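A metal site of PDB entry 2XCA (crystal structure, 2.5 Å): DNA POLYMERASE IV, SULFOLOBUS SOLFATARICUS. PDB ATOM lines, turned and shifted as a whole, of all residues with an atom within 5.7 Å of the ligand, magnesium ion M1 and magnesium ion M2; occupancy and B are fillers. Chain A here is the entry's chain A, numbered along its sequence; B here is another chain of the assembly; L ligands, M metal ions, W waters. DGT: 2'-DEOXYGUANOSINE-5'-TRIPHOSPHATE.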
ATOM      1  N   PHE A  11      -1.049  -7.031  -7.496  1.00  0.00           N
ATOM      2  CA  PHE A  11      -2.371  -6.484  -7.787  1.00  0.00           C
ATOM      3  C   PHE A  11      -2.233  -5.098  -8.409  1.00  0.00           C
ATOM      4  O   PHE A  11      -1.419  -4.279  -7.978  1.00  0.00           O
ATOM      5  CB  PHE A  11      -3.179  -6.404  -6.479  1.00  0.00           C
ATOM      6  CG  PHE A  11      -4.399  -5.523  -6.558  1.00  0.00           C
ATOM      7  CD1 PHE A  11      -5.615  -6.014  -7.051  1.00  0.00           C
ATOM      8  CD2 PHE A  11      -4.355  -4.206  -6.074  1.00  0.00           C
ATOM      9  CE1 PHE A  11      -6.770  -5.199  -7.057  1.00  0.00           C
ATOM     10  CE2 PHE A  11      -5.495  -3.406  -6.091  1.00  0.00           C
ATOM     11  CZ  PHE A  11      -6.714  -3.900  -6.576  1.00  0.00           C
ATOM     12  N   ASP A  13      -4.456  -1.623  -9.859  1.00  0.00           N
ATOM     13  CA  ASP A  13      -5.698  -0.867  -9.808  1.00  0.00           C
ATOM     14  C   ASP A  13      -5.491   0.495 -10.501  1.00  0.00           C
ATOM     15  O   ASP A  13      -4.607   1.246 -10.110  1.00  0.00           O
ATOM     16  CB  ASP A  13      -6.109  -0.667  -8.365  1.00  0.00           C
ATOM     17  CG  ASP A  13      -7.537  -0.170  -8.241  1.00  0.00           C
ATOM     18  OD1 ASP A  13      -8.445  -1.009  -8.276  1.00  0.00           O
ATOM     19  OD2 ASP A  13      -7.724   1.052  -8.123  1.00  0.00           O
ATOM     20  N   PHE A  14      -6.310   0.807 -11.508  1.00  0.00           N
ATOM     21  CA  PHE A  14      -6.164   2.069 -12.237  1.00  0.00           C
ATOM     22  C   PHE A  14      -6.548   3.283 -11.374  1.00  0.00           C
ATOM     23  O   PHE A  14      -7.528   3.256 -10.671  1.00  0.00           O
ATOM     24  CB  PHE A  14      -7.013   2.065 -13.513  1.00  0.00           C
ATOM     25  CG  PHE A  14      -6.939   0.777 -14.277  1.00  0.00           C
ATOM     26  CD1 PHE A  14      -5.899  -0.119 -14.062  1.00  0.00           C
ATOM     27  CD2 PHE A  14      -7.937   0.450 -15.180  1.00  0.00           C
ATOM     28  CE1 PHE A  14      -5.856  -1.342 -14.749  1.00  0.00           C
ATOM     29  CE2 PHE A  14      -7.914  -0.749 -15.868  1.00  0.00           C
ATOM     30  CZ  PHE A  14      -6.866  -1.672 -15.658  1.00  0.00           C
ATOM     31  N   ASP A  15      -5.794   4.372 -11.440  1.00  0.00           N
ATOM     32  CA  ASP A  15      -6.124   5.513 -10.615  1.00  0.00           C
ATOM     33  C   ASP A  15      -7.356   6.292 -11.085  1.00  0.00           C
ATOM     34  O   ASP A  15      -7.529   6.501 -12.284  1.00  0.00           O
ATOM     35  CB  ASP A  15      -4.911   6.428 -10.498  1.00  0.00           C
ATOM     36  CG  ASP A  15      -3.753   5.746  -9.787  1.00  0.00           C
ATOM     37  OD1 ASP A  15      -3.998   4.833  -8.966  1.00  0.00           O
ATOM     38  OD2 ASP A  15      -2.595   6.124 -10.025  1.00  0.00           O
ATOM     39  N   TYR A  16      -8.204   6.707 -10.142  1.00  0.00           N
ATOM     40  CA  TYR A  16      -9.444   7.463 -10.452  1.00  0.00           C
ATOM     41  C   TYR A  16      -9.851   7.223 -11.890  1.00  0.00           C
ATOM     42  O   TYR A  16     -10.135   8.144 -12.651  1.00  0.00           O
ATOM     43  CB  TYR A  16      -9.226   8.972 -10.161  1.00  0.00           C
ATOM     44  CG  TYR A  16      -8.110   9.651 -10.947  1.00  0.00           C
ATOM     45  CD1 TYR A  16      -8.402  10.403 -12.098  1.00  0.00           C
ATOM     46  CD2 TYR A  16      -6.778   9.549 -10.543  1.00  0.00           C
ATOM     47  CE1 TYR A  16      -7.405  11.032 -12.813  1.00  0.00           C
ATOM     48  CE2 TYR A  16      -5.769  10.192 -11.271  1.00  0.00           C
ATOM     49  CZ  TYR A  16      -6.089  10.924 -12.407  1.00  0.00           C
ATOM     50  OH  TYR A  16      -5.091  11.526 -13.165  1.00  0.00           O
ATOM     51  N   PHE A  17      -9.923   5.939 -12.226  1.00  0.00           N
ATOM     52  CA  PHE A  17     -10.212   5.431 -13.561  1.00  0.00           C
ATOM     53  C   PHE A  17     -11.156   6.128 -14.531  1.00  0.00           C
ATOM     54  O   PHE A  17     -10.693   6.562 -15.587  1.00  0.00           O
ATOM     55  CB  PHE A  17     -10.567   3.940 -13.482  1.00  0.00           C
ATOM     56  CG  PHE A  17     -10.543   3.245 -14.822  1.00  0.00           C
ATOM     57  CD1 PHE A  17      -9.469   3.404 -15.691  1.00  0.00           C
ATOM     58  CD2 PHE A  17     -11.608   2.458 -15.220  1.00  0.00           C
ATOM     59  CE1 PHE A  17      -9.455   2.790 -16.939  1.00  0.00           C
ATOM     60  CE2 PHE A  17     -11.615   1.831 -16.470  1.00  0.00           C
ATOM     61  CZ  PHE A  17     -10.532   2.006 -17.329  1.00  0.00           C
ATOM     62  N   TYR A  18     -12.441   6.232 -14.224  1.00  0.00           N
ATOM     63  CA  TYR A  18     -13.369   6.869 -15.174  1.00  0.00           C
ATOM     64  C   TYR A  18     -12.994   8.299 -15.458  1.00  0.00           C
ATOM     65  O   TYR A  18     -13.107   8.780 -16.584  1.00  0.00           O
ATOM     66  CB  TYR A  18     -14.800   6.854 -14.627  1.00  0.00           C
ATOM     67  CG  TYR A  18     -15.487   5.516 -14.642  1.00  0.00           C
ATOM     68  CD1 TYR A  18     -14.767   4.348 -14.820  1.00  0.00           C
ATOM     69  CD2 TYR A  18     -16.856   5.419 -14.416  1.00  0.00           C
ATOM     70  CE1 TYR A  18     -15.401   3.098 -14.795  1.00  0.00           C
ATOM     71  CE2 TYR A  18     -17.494   4.205 -14.380  1.00  0.00           C
ATOM     72  CZ  TYR A  18     -16.770   3.039 -14.567  1.00  0.00           C
ATOM     73  OH  TYR A  18     -17.392   1.829 -14.534  1.00  0.00           O
ATOM     74  N   ALA A  19     -12.550   9.012 -14.431  1.00  0.00           N
ATOM     75  CA  ALA A  19     -12.167  10.398 -14.580  1.00  0.00           C
ATOM     76  C   ALA A  19     -10.888  10.473 -15.417  1.00  0.00           C
ATOM     77  O   ALA A  19     -10.804  11.252 -16.383  1.00  0.00           O
ATOM     78  CB  ALA A  19     -11.979  11.032 -13.231  1.00  0.00           C
ATOM     79  N   VAL A  38     -23.510  10.041 -12.851  1.00  0.00           N
ATOM     80  CA  VAL A  38     -24.549   9.179 -13.343  1.00  0.00           C
ATOM     81  C   VAL A  38     -25.848   9.955 -13.094  1.00  0.00           C
ATOM     82  O   VAL A  38     -26.395   9.920 -11.979  1.00  0.00           O
ATOM     83  CB  VAL A  38     -24.572   7.833 -12.592  1.00  0.00           C
ATOM     84  CG1 VAL A  38     -25.794   7.023 -13.017  1.00  0.00           C
ATOM     85  CG2 VAL A  38     -23.317   7.077 -12.854  1.00  0.00           C
ATOM     86  N   VAL A  49     -22.327  10.461  -8.000  1.00  0.00           N
ATOM     87  CA  VAL A  49     -21.025  10.557  -8.605  1.00  0.00           C
ATOM     88  C   VAL A  49     -20.413   9.175  -8.776  1.00  0.00           C
ATOM     89  O   VAL A  49     -20.291   8.431  -7.805  1.00  0.00           O
ATOM     90  CB  VAL A  49     -20.078  11.403  -7.725  1.00  0.00           C
ATOM     91  CG1 VAL A  49     -18.655  11.283  -8.253  1.00  0.00           C
ATOM     92  CG2 VAL A  49     -20.539  12.862  -7.704  1.00  0.00           C
ATOM     93  N   ALA A  50     -20.036   8.818 -10.003  1.00  0.00           N
ATOM     94  CA  ALA A  50     -19.402   7.503 -10.245  1.00  0.00           C
ATOM     95  C   ALA A  50     -18.008   7.525  -9.649  1.00  0.00           C
ATOM     96  O   ALA A  50     -17.599   6.569  -8.974  1.00  0.00           O
ATOM     97  CB  ALA A  50     -19.322   7.201 -11.721  1.00  0.00           C
ATOM     98  N   THR A  51     -17.287   8.609  -9.900  1.00  0.00           N
ATOM     99  CA  THR A  51     -15.944   8.864  -9.368  1.00  0.00           C
ATOM    100  C   THR A  51     -15.459  10.275  -9.728  1.00  0.00           C
ATOM    101  O   THR A  51     -16.062  10.963 -10.528  1.00  0.00           O
ATOM    102  CB  THR A  51     -14.883   7.879  -9.889  1.00  0.00           C
ATOM    103  OG1 THR A  51     -13.712   7.956  -9.058  1.00  0.00           O
ATOM    104  CG2 THR A  51     -14.473   8.217 -11.351  1.00  0.00           C
ATOM    105  N   ALA A  52     -14.340  10.685  -9.132  1.00  0.00           N
ATOM    106  CA  ALA A  52     -13.768  11.999  -9.387  1.00  0.00           C
ATOM    107  C   ALA A  52     -12.258  11.898  -9.296  1.00  0.00           C
ATOM    108  O   ALA A  52     -11.758  11.063  -8.542  1.00  0.00           O
ATOM    109  CB  ALA A  52     -14.254  12.995  -8.358  1.00  0.00           C
ATOM    110  N   TYR A  54      -8.418  13.041  -8.238  1.00  0.00           N
ATOM    111  CA  TYR A  54      -7.942  13.413  -6.897  1.00  0.00           C
ATOM    112  C   TYR A  54      -8.064  14.885  -6.541  1.00  0.00           C
ATOM    113  O   TYR A  54      -8.199  15.226  -5.368  1.00  0.00           O
ATOM    114  CB  TYR A  54      -6.502  12.911  -6.689  1.00  0.00           C
ATOM    115  CG  TYR A  54      -6.455  11.409  -6.451  1.00  0.00           C
ATOM    116  CD1 TYR A  54      -6.781  10.515  -7.458  1.00  0.00           C
ATOM    117  CD2 TYR A  54      -6.130  10.915  -5.198  1.00  0.00           C
ATOM    118  CE1 TYR A  54      -6.778   9.145  -7.227  1.00  0.00           C
ATOM    119  CE2 TYR A  54      -6.122   9.541  -4.943  1.00  0.00           C
ATOM    120  CZ  TYR A  54      -6.449   8.658  -5.969  1.00  0.00           C
ATOM    121  OH  TYR A  54      -6.414   7.294  -5.757  1.00  0.00           O
ATOM    122  N   ARG A  57     -11.332  15.022  -5.068  1.00  0.00           N
ATOM    123  CA  ARG A  57     -11.510  14.245  -3.833  1.00  0.00           C
ATOM    124  C   ARG A  57     -10.976  14.961  -2.610  1.00  0.00           C
ATOM    125  O   ARG A  57     -11.316  14.605  -1.477  1.00  0.00           O
ATOM    126  CB  ARG A  57     -10.814  12.882  -3.918  1.00  0.00           C
ATOM    127  CG  ARG A  57     -11.441  11.909  -4.893  1.00  0.00           C
ATOM    128  CD  ARG A  57     -10.765  10.558  -4.824  1.00  0.00           C
ATOM    129  NE  ARG A  57     -11.044   9.789  -6.029  1.00  0.00           N
ATOM    130  CZ  ARG A  57     -10.614   8.540  -6.251  1.00  0.00           C
ATOM    131  NH1 ARG A  57      -9.888   7.925  -5.318  1.00  0.00           N
ATOM    132  NH2 ARG A  57     -10.909   7.927  -7.398  1.00  0.00           N
ATOM    133  N   ALA A  63     -17.099   9.082  -5.208  1.00  0.00           N
ATOM    134  CA  ALA A  63     -18.089   8.079  -5.615  1.00  0.00           C
ATOM    135  C   ALA A  63     -19.120   7.846  -4.505  1.00  0.00           C
ATOM    136  O   ALA A  63     -18.777   7.701  -3.340  1.00  0.00           O
ATOM    137  CB  ALA A  63     -17.379   6.762  -5.951  1.00  0.00           C
ATOM    138  N   GLY A  64     -20.386   7.835  -4.888  1.00  0.00           N
ATOM    139  CA  GLY A  64     -21.443   7.599  -3.925  1.00  0.00           C
ATOM    140  C   GLY A  64     -22.289   8.797  -3.539  1.00  0.00           C
ATOM    141  O   GLY A  64     -23.510   8.660  -3.413  1.00  0.00           O
ATOM    142  N   MET A  82     -21.177   9.838 -17.151  1.00  0.00           N
ATOM    143  CA  MET A  82     -20.452   8.574 -17.236  1.00  0.00           C
ATOM    144  C   MET A  82     -20.634   7.876 -18.592  1.00  0.00           C
ATOM    145  O   MET A  82     -21.759   7.641 -19.039  1.00  0.00           O
ATOM    146  CB  MET A  82     -20.916   7.629 -16.118  1.00  0.00           C
ATOM    147  CG  MET A  82     -20.243   6.264 -16.157  1.00  0.00           C
ATOM    148  SD  MET A  82     -20.962   5.151 -14.986  1.00  0.00           S
ATOM    149  CE  MET A  82     -22.456   4.632 -15.873  1.00  0.00           C
ATOM    150  N   SER A 109     -12.578  -6.426 -11.164  1.00  0.00           N
ATOM    151  CA  SER A 109     -13.497  -5.310 -11.368  1.00  0.00           C
ATOM    152  C   SER A 109     -13.146  -4.680 -12.696  1.00  0.00           C
ATOM    153  O   SER A 109     -12.290  -5.189 -13.419  1.00  0.00           O
ATOM    154  CB  SER A 109     -13.324  -4.255 -10.265  1.00  0.00           C
ATOM    155  OG  SER A 109     -12.271  -3.343 -10.566  1.00  0.00           O
ATOM    156  N   ILE A 110     -13.812  -3.582 -13.030  1.00  0.00           N
ATOM    157  CA  ILE A 110     -13.531  -2.912 -14.294  1.00  0.00           C
ATOM    158  C   ILE A 110     -12.159  -2.263 -14.295  1.00  0.00           C
ATOM    159  O   ILE A 110     -11.687  -1.813 -15.342  1.00  0.00           O
ATOM    160  CB  ILE A 110     -14.570  -1.854 -14.589  1.00  0.00           C
ATOM    161  CG1 ILE A 110     -14.424  -1.377 -16.031  1.00  0.00           C
ATOM    162  CG2 ILE A 110     -14.400  -0.693 -13.622  1.00  0.00           C
ATOM    163  CD1 ILE A 110     -15.663  -0.685 -16.590  1.00  0.00           C
ATOM    164  N   ASP A 111     -11.480  -2.203 -13.149  1.00  0.00           N
ATOM    165  CA  ASP A 111     -10.155  -1.555 -13.170  1.00  0.00           C
ATOM    166  C   ASP A 111      -9.109  -2.175 -12.278  1.00  0.00           C
ATOM    167  O   ASP A 111      -8.159  -1.489 -11.883  1.00  0.00           O
ATOM    168  CB  ASP A 111     -10.290  -0.069 -12.825  1.00  0.00           C
ATOM    169  CG  ASP A 111     -10.399   0.140 -11.336  1.00  0.00           C
ATOM    170  OD1 ASP A 111     -11.123  -0.645 -10.688  1.00  0.00           O
ATOM    171  OD2 ASP A 111      -9.776   1.092 -10.834  1.00  0.00           O
ATOM    172  N   GLU A 112      -9.259  -3.459 -11.955  1.00  0.00           N
ATOM    173  CA  GLU A 112      -8.261  -4.110 -11.117  1.00  0.00           C
ATOM    174  C   GLU A 112      -8.103  -5.602 -11.408  1.00  0.00           C
ATOM    175  O   GLU A 112      -9.044  -6.294 -11.802  1.00  0.00           O
ATOM    176  CB  GLU A 112      -8.554  -3.887  -9.629  1.00  0.00           C
ATOM    177  CG  GLU A 112      -9.885  -4.426  -9.166  1.00  0.00           C
ATOM    178  CD  GLU A 112     -10.383  -3.730  -7.893  1.00  0.00           C
ATOM    179  OE1 GLU A 112     -10.004  -4.104  -6.769  1.00  0.00           O
ATOM    180  OE2 GLU A 112     -11.157  -2.781  -8.039  1.00  0.00           O
ATOM    181  N   LYS A 158      -3.900  -6.192  -2.314  1.00  0.00           N
ATOM    182  CA  LYS A 158      -4.908  -5.146  -2.419  1.00  0.00           C
ATOM    183  C   LYS A 158      -4.613  -4.038  -1.396  1.00  0.00           C
ATOM    184  O   LYS A 158      -4.630  -2.857  -1.710  1.00  0.00           O
ATOM    185  CB  LYS A 158      -6.293  -5.750  -2.170  1.00  0.00           C
ATOM    186  CG  LYS A 158      -7.439  -4.758  -2.044  1.00  0.00           C
ATOM    187  CD  LYS A 158      -7.710  -4.046  -3.326  1.00  0.00           C
ATOM    188  CE  LYS A 158      -8.847  -3.035  -3.178  1.00  0.00           C
ATOM    189  NZ  LYS A 158      -9.092  -2.260  -4.438  1.00  0.00           N
ATOM    190  N   LYS A 165      -1.818   4.381  -3.071  1.00  0.00           N
ATOM    191  CA  LYS A 165      -2.595   5.213  -3.994  1.00  0.00           C
ATOM    192  C   LYS A 165      -2.247   6.695  -3.784  1.00  0.00           C
ATOM    193  O   LYS A 165      -2.118   7.133  -2.640  1.00  0.00           O
ATOM    194  CB  LYS A 165      -4.092   5.002  -3.757  1.00  0.00           C
ATOM    195  CG  LYS A 165      -4.709   3.767  -4.399  1.00  0.00           C
ATOM    196  CD  LYS A 165      -5.041   4.014  -5.865  1.00  0.00           C
ATOM    197  CE  LYS A 165      -5.631   2.773  -6.544  1.00  0.00           C
ATOM    198  NZ  LYS A 165      -5.994   3.020  -7.977  1.00  0.00           N
ATOM    199  N   PRO A 166      -2.093   7.476  -4.869  1.00  0.00           N
ATOM    200  CA  PRO A 166      -2.218   7.101  -6.284  1.00  0.00           C
ATOM    201  C   PRO A 166      -0.857   6.980  -6.951  1.00  0.00           C
ATOM    202  O   PRO A 166       0.172   7.327  -6.357  1.00  0.00           O
ATOM    203  CB  PRO A 166      -3.033   8.241  -6.856  1.00  0.00           C
ATOM    204  CG  PRO A 166      -2.445   9.414  -6.145  1.00  0.00           C
ATOM    205  CD  PRO A 166      -2.277   8.932  -4.713  1.00  0.00           C
ATOM    206  P    DC B   4     -29.985   6.721  -6.495  1.00  0.00           P
ATOM    207  OP1  DC B   4     -31.374   7.253  -6.672  1.00  0.00           O
ATOM    208  OP2  DC B   4     -29.715   5.631  -5.538  1.00  0.00           O
ATOM    209  O5'  DC B   4     -29.361   6.378  -7.901  1.00  0.00           O
ATOM    210  C5'  DC B   4     -29.182   7.459  -8.815  1.00  0.00           C
ATOM    211  C4'  DC B   4     -28.273   7.042  -9.972  1.00  0.00           C
ATOM    212  O4'  DC B   4     -26.911   6.832  -9.525  1.00  0.00           O
ATOM    213  C3'  DC B   4     -28.725   5.669 -10.493  1.00  0.00           C
ATOM    214  O3'  DC B   4     -28.568   5.664 -11.892  1.00  0.00           O
ATOM    215  C2'  DC B   4     -27.788   4.688  -9.805  1.00  0.00           C
ATOM    216  C1'  DC B   4     -26.516   5.483  -9.717  1.00  0.00           C
ATOM    217  N1   DC B   4     -25.630   5.136  -8.604  1.00  0.00           N
ATOM    218  C2   DC B   4     -24.324   4.744  -8.878  1.00  0.00           C
ATOM    219  O2   DC B   4     -23.979   4.644 -10.052  1.00  0.00           O
ATOM    220  N3   DC B   4     -23.464   4.495  -7.866  1.00  0.00           N
ATOM    221  C4   DC B   4     -23.881   4.642  -6.591  1.00  0.00           C
ATOM    222  N4   DC B   4     -22.986   4.451  -5.625  1.00  0.00           N
ATOM    223  C5   DC B   4     -25.221   4.992  -6.278  1.00  0.00           C
ATOM    224  C6   DC B   4     -26.058   5.220  -7.299  1.00  0.00           C
ATOM    225  P   8OG B   5     -29.448   4.661 -12.788  1.00  0.00           P
ATOM    226  OP1 8OG B   5     -29.539   5.178 -14.177  1.00  0.00           O
ATOM    227  OP2 8OG B   5     -30.698   4.368 -12.049  1.00  0.00           O
ATOM    228  O5' 8OG B   5     -28.557   3.345 -12.835  1.00  0.00           O
ATOM    229  C5' 8OG B   5     -27.250   3.438 -13.416  1.00  0.00           C
ATOM    230  C4' 8OG B   5     -26.335   2.385 -12.807  1.00  0.00           C
ATOM    231  O4' 8OG B   5     -26.227   2.519 -11.380  1.00  0.00           O
ATOM    232  C3' 8OG B   5     -26.844   0.958 -12.996  1.00  0.00           C
ATOM    233  O3' 8OG B   5     -26.285   0.436 -14.229  1.00  0.00           O
ATOM    234  C2' 8OG B   5     -26.314   0.218 -11.766  1.00  0.00           C
ATOM    235  C1' 8OG B   5     -25.544   1.312 -11.009  1.00  0.00           C
ATOM    236  N9  8OG B   5     -25.514   1.180  -9.535  1.00  0.00           N
ATOM    237  C8  8OG B   5     -26.547   1.252  -8.706  1.00  0.00           C
ATOM    238  N7  8OG B   5     -26.155   1.299  -7.432  1.00  0.00           N
ATOM    239  C5  8OG B   5     -24.837   1.225  -7.466  1.00  0.00           C
ATOM    240  C6  8OG B   5     -23.908   1.210  -6.437  1.00  0.00           C
ATOM    241  O6  8OG B   5     -24.216   1.333  -5.251  1.00  0.00           O
ATOM    242  N1  8OG B   5     -22.569   1.097  -6.804  1.00  0.00           N
ATOM    243  C2  8OG B   5     -22.201   1.022  -8.154  1.00  0.00           C
ATOM    244  N2  8OG B   5     -20.933   0.902  -8.485  1.00  0.00           N
ATOM    245  N3  8OG B   5     -23.127   1.034  -9.137  1.00  0.00           N
ATOM    246  C4  8OG B   5     -24.398   1.134  -8.792  1.00  0.00           C
ATOM    247  O8  8OG B   5     -27.701   1.273  -9.122  1.00  0.00           O
HETATM  248  PG  DGT L   1      -8.832   4.939  -7.142  1.00  0.00           P
HETATM  249  O1G DGT L   1      -8.943   5.239  -5.566  1.00  0.00           O
HETATM  250  O2G DGT L   1      -9.054   3.351  -7.293  1.00  0.00           O
HETATM  251  O3G DGT L   1      -7.532   5.391  -7.694  1.00  0.00           O
HETATM  252  O3B DGT L   1     -10.094   5.653  -7.828  1.00  0.00           O
HETATM  253  PB  DGT L   1     -11.154   4.866  -8.744  1.00  0.00           P
HETATM  254  O1B DGT L   1     -12.067   5.879  -9.310  1.00  0.00           O
HETATM  255  O2B DGT L   1     -10.424   3.986  -9.680  1.00  0.00           O
HETATM  256  O3A DGT L   1     -11.945   3.990  -7.646  1.00  0.00           O
HETATM  257  PA  DGT L   1     -11.902   2.384  -7.581  1.00  0.00           P
HETATM  258  O1A DGT L   1     -10.702   1.722  -8.421  1.00  0.00           O
HETATM  259  O2A DGT L   1     -12.522   1.662  -6.451  1.00  0.00           O
HETATM  260  O5' DGT L   1     -13.049   2.179  -8.684  1.00  0.00           O
HETATM  261  C5' DGT L   1     -12.737   2.136 -10.079  1.00  0.00           C
HETATM  262  C4' DGT L   1     -13.920   2.637 -10.920  1.00  0.00           C
HETATM  263  O4' DGT L   1     -15.139   1.912 -10.690  1.00  0.00           O
HETATM  264  C3' DGT L   1     -14.291   4.088 -10.615  1.00  0.00           C
HETATM  265  O3' DGT L   1     -13.374   4.958 -11.269  1.00  0.00           O
HETATM  266  C2' DGT L   1     -15.628   4.131 -11.358  1.00  0.00           C
HETATM  267  C1' DGT L   1     -16.248   2.805 -10.878  1.00  0.00           C
HETATM  268  N9  DGT L   1     -16.929   2.999  -9.581  1.00  0.00           N
HETATM  269  C8  DGT L   1     -16.411   2.838  -8.361  1.00  0.00           C
HETATM  270  N7  DGT L   1     -17.331   3.087  -7.436  1.00  0.00           N
HETATM  271  C5  DGT L   1     -18.466   3.387  -8.066  1.00  0.00           C
HETATM  272  C6  DGT L   1     -19.734   3.753  -7.627  1.00  0.00           C
HETATM  273  O6  DGT L   1     -20.012   3.818  -6.415  1.00  0.00           O
HETATM  274  N1  DGT L   1     -20.721   4.043  -8.585  1.00  0.00           N
HETATM  275  C2  DGT L   1     -20.407   3.976  -9.942  1.00  0.00           C
HETATM  276  N2  DGT L   1     -21.322   4.298 -10.848  1.00  0.00           N
HETATM  277  N3  DGT L   1     -19.165   3.622 -10.330  1.00  0.00           N
HETATM  278  C4  DGT L   1     -18.206   3.346  -9.436  1.00  0.00           C
HETATM  279 MG    MG M   1      -8.850   2.587  -9.297  1.00  0.00          MG
HETATM  280 MG    MG M   2     -10.529  -0.706  -8.689  1.00  0.00          MG
HETATM  281  O   HOH W   1     -19.627   2.098 -12.969  1.00  0.00           O
HETATM  282  O   HOH W   2     -20.917   1.464  -4.002  1.00  0.00           O
HETATM  283  O   HOH W   3     -19.304   3.857  -3.361  1.00  0.00           O
HETATM  284  O   HOH W   4     -10.414  -0.459  -6.461  1.00  0.00           O
HETATM  285  O   HOH W   5     -12.803  -0.758  -8.407  1.00  0.00           O
HETATM  286  O   HOH W   6      -8.513   1.761  -5.491  1.00  0.00           O
HETATM  287  O   HOH W   7     -15.292  -0.981 -10.118  1.00  0.00           O
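The guanidinium group of Arg 57 is in salt-bridge range of an oxygen (O1G) of the ligand (2.9 Å).
The side-chain hydroxyl (OH) of Tyr 54 sits at hydrogen-bond distance from an oxygen (O3G) of the ligand, at 2.9 Å.
The side-chain hydroxyl (OG1) of Thr 51 is in hydrogen-bond range of an oxygen (O1B) of the ligand (2.7 Å).
An oxygen (O2B) of the ligand lies close to the backbone NH (N) of Phe 17 (3.2 Å).
N of Tyr 16 lies within hydrogen-bond range of O3G of the ligand (2.9 Å).
The side-chain amino group of Lys 165 lies within salt-bridge range of an oxygen (O3G) of the ligand (2.8 Å).
The backbone NH (N) of Tyr 18 sits at hydrogen-bond distance from an oxygen (O3') of the ligand (3.4 Å).
O2 of DC 4 of chain B lies within hydrogen-bond range of N2 of the ligand, 2.8 Å away.
N1 of the ligand lies within hydrogen-bond range of N2 of 8OG 5 of chain B (3.1 Å).
The guanidinium group of Arg 57 is in hydrogen-bond range of the side-chain hydroxyl of Thr 51 (3.3 Å).
O of Phe 14 sits close to NZ of Lys 165 (3.1 Å).
OD1 of Asp 15 is in salt-bridge range of NZ of Lys 165 (2.9 Å).
The guanidinium group (NE) of Arg 57 is in hydrogen-bond range of the backbone carbonyl oxygen (O) of Ala 52.
The side-chain carboxylate (OE1) of Glu 112 lies within salt-bridge range of the side-chain amino group (NZ) of Lys 158 (3.1 Å).
NZ of Lys 165 is in hydrogen-bond range of O of Asp 13 (3.1 Å).
N of Asp 111 is in hydrogen-bond range of OG of Ser 109 (2.9 Å).
N of Glu 112 sits close to OG of Ser 109, at 3.3 Å.
Asp 15 touches the ligand (CA to O3G, 3.2 Å).
Val 38 touches the ligand (CG2 to N2, 3.97 Å).
Ala 50 touches the ligand (O to C4, 3.3 Å).
CB of Ala 63 touches N7 of the ligand, at 3.96 Å.
Ile 110 touches the ligand.
Hydrophobic or aromatic side chains within 4 Å of the ligand: Phe 17, Tyr 18, Val 38, Ala 50, Tyr 54, Ala 63 and Ile 110.
Within 4 Å of the ligand: Asp 13, Phe 14, Asp 15, Tyr 16, Phe 17, Tyr 18, Val 38, Ala 50, Thr 51, Tyr 54, Arg 57, Ala 63, Ile 110, Asp 111, Lys 165, DC 4 of chain B and 8OG 5 of chain B.
The nearest printed residue that does not touch the ligand is Met 82 (4.2 Å).
Residues that only touch magnesium ion M1: Lys 165.
Four residues have an atom within 4 Å of magnesium ion M1: Asp 13, Phe 14, Asp 111 and Lys 165.
Merely in contact with magnesium ion M2: Ser 109.
Of the 27 residues printed, 4 come within 4 Å of magnesium ion M2.
Magnesium ion M1 is bound by the backbone carbonyl oxygen (O) of Phe 14, an oxygen (O2B) of the ligand, an oxygen (O2G) of the ligand, an oxygen (O1A) of the ligand, the side-chain carboxylate (OD2) of Asp 13 and the side-chain carboxylate (OD2) of Asp 111.
Magnesium ion M1 has six donor atoms within binding distance.
Magnesium ion M2 is bound by the side-chain carboxylate of Asp 111 (2.1 Å), the side-chain carboxylate of Asp 13 (2.1 Å), water W4 (2.2 Å), the side-chain carboxylate of Glu 112 (2.3 Å), water W5 (2.3 Å) and an oxygen (O1A) of the ligand (2.4 Å).
Magnesium ion M2 has six donor atoms within binding distance.
Water W4 lies within hydrogen-bond range of O2A of the ligand (3.0 Å) and NZ of Lys 158 (3.0 Å).
Water W5 bridges O5' of the ligand (3.0 Å) and OG of Ser 109 (3.4 Å).
Water W1 lies within hydrogen-bond range of the side-chain hydroxyl of Tyr 18 and a nitrogen (N3) of the ligand.
Water W2 bridges N1 of 8OG 5 of chain B and O6 of the ligand.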
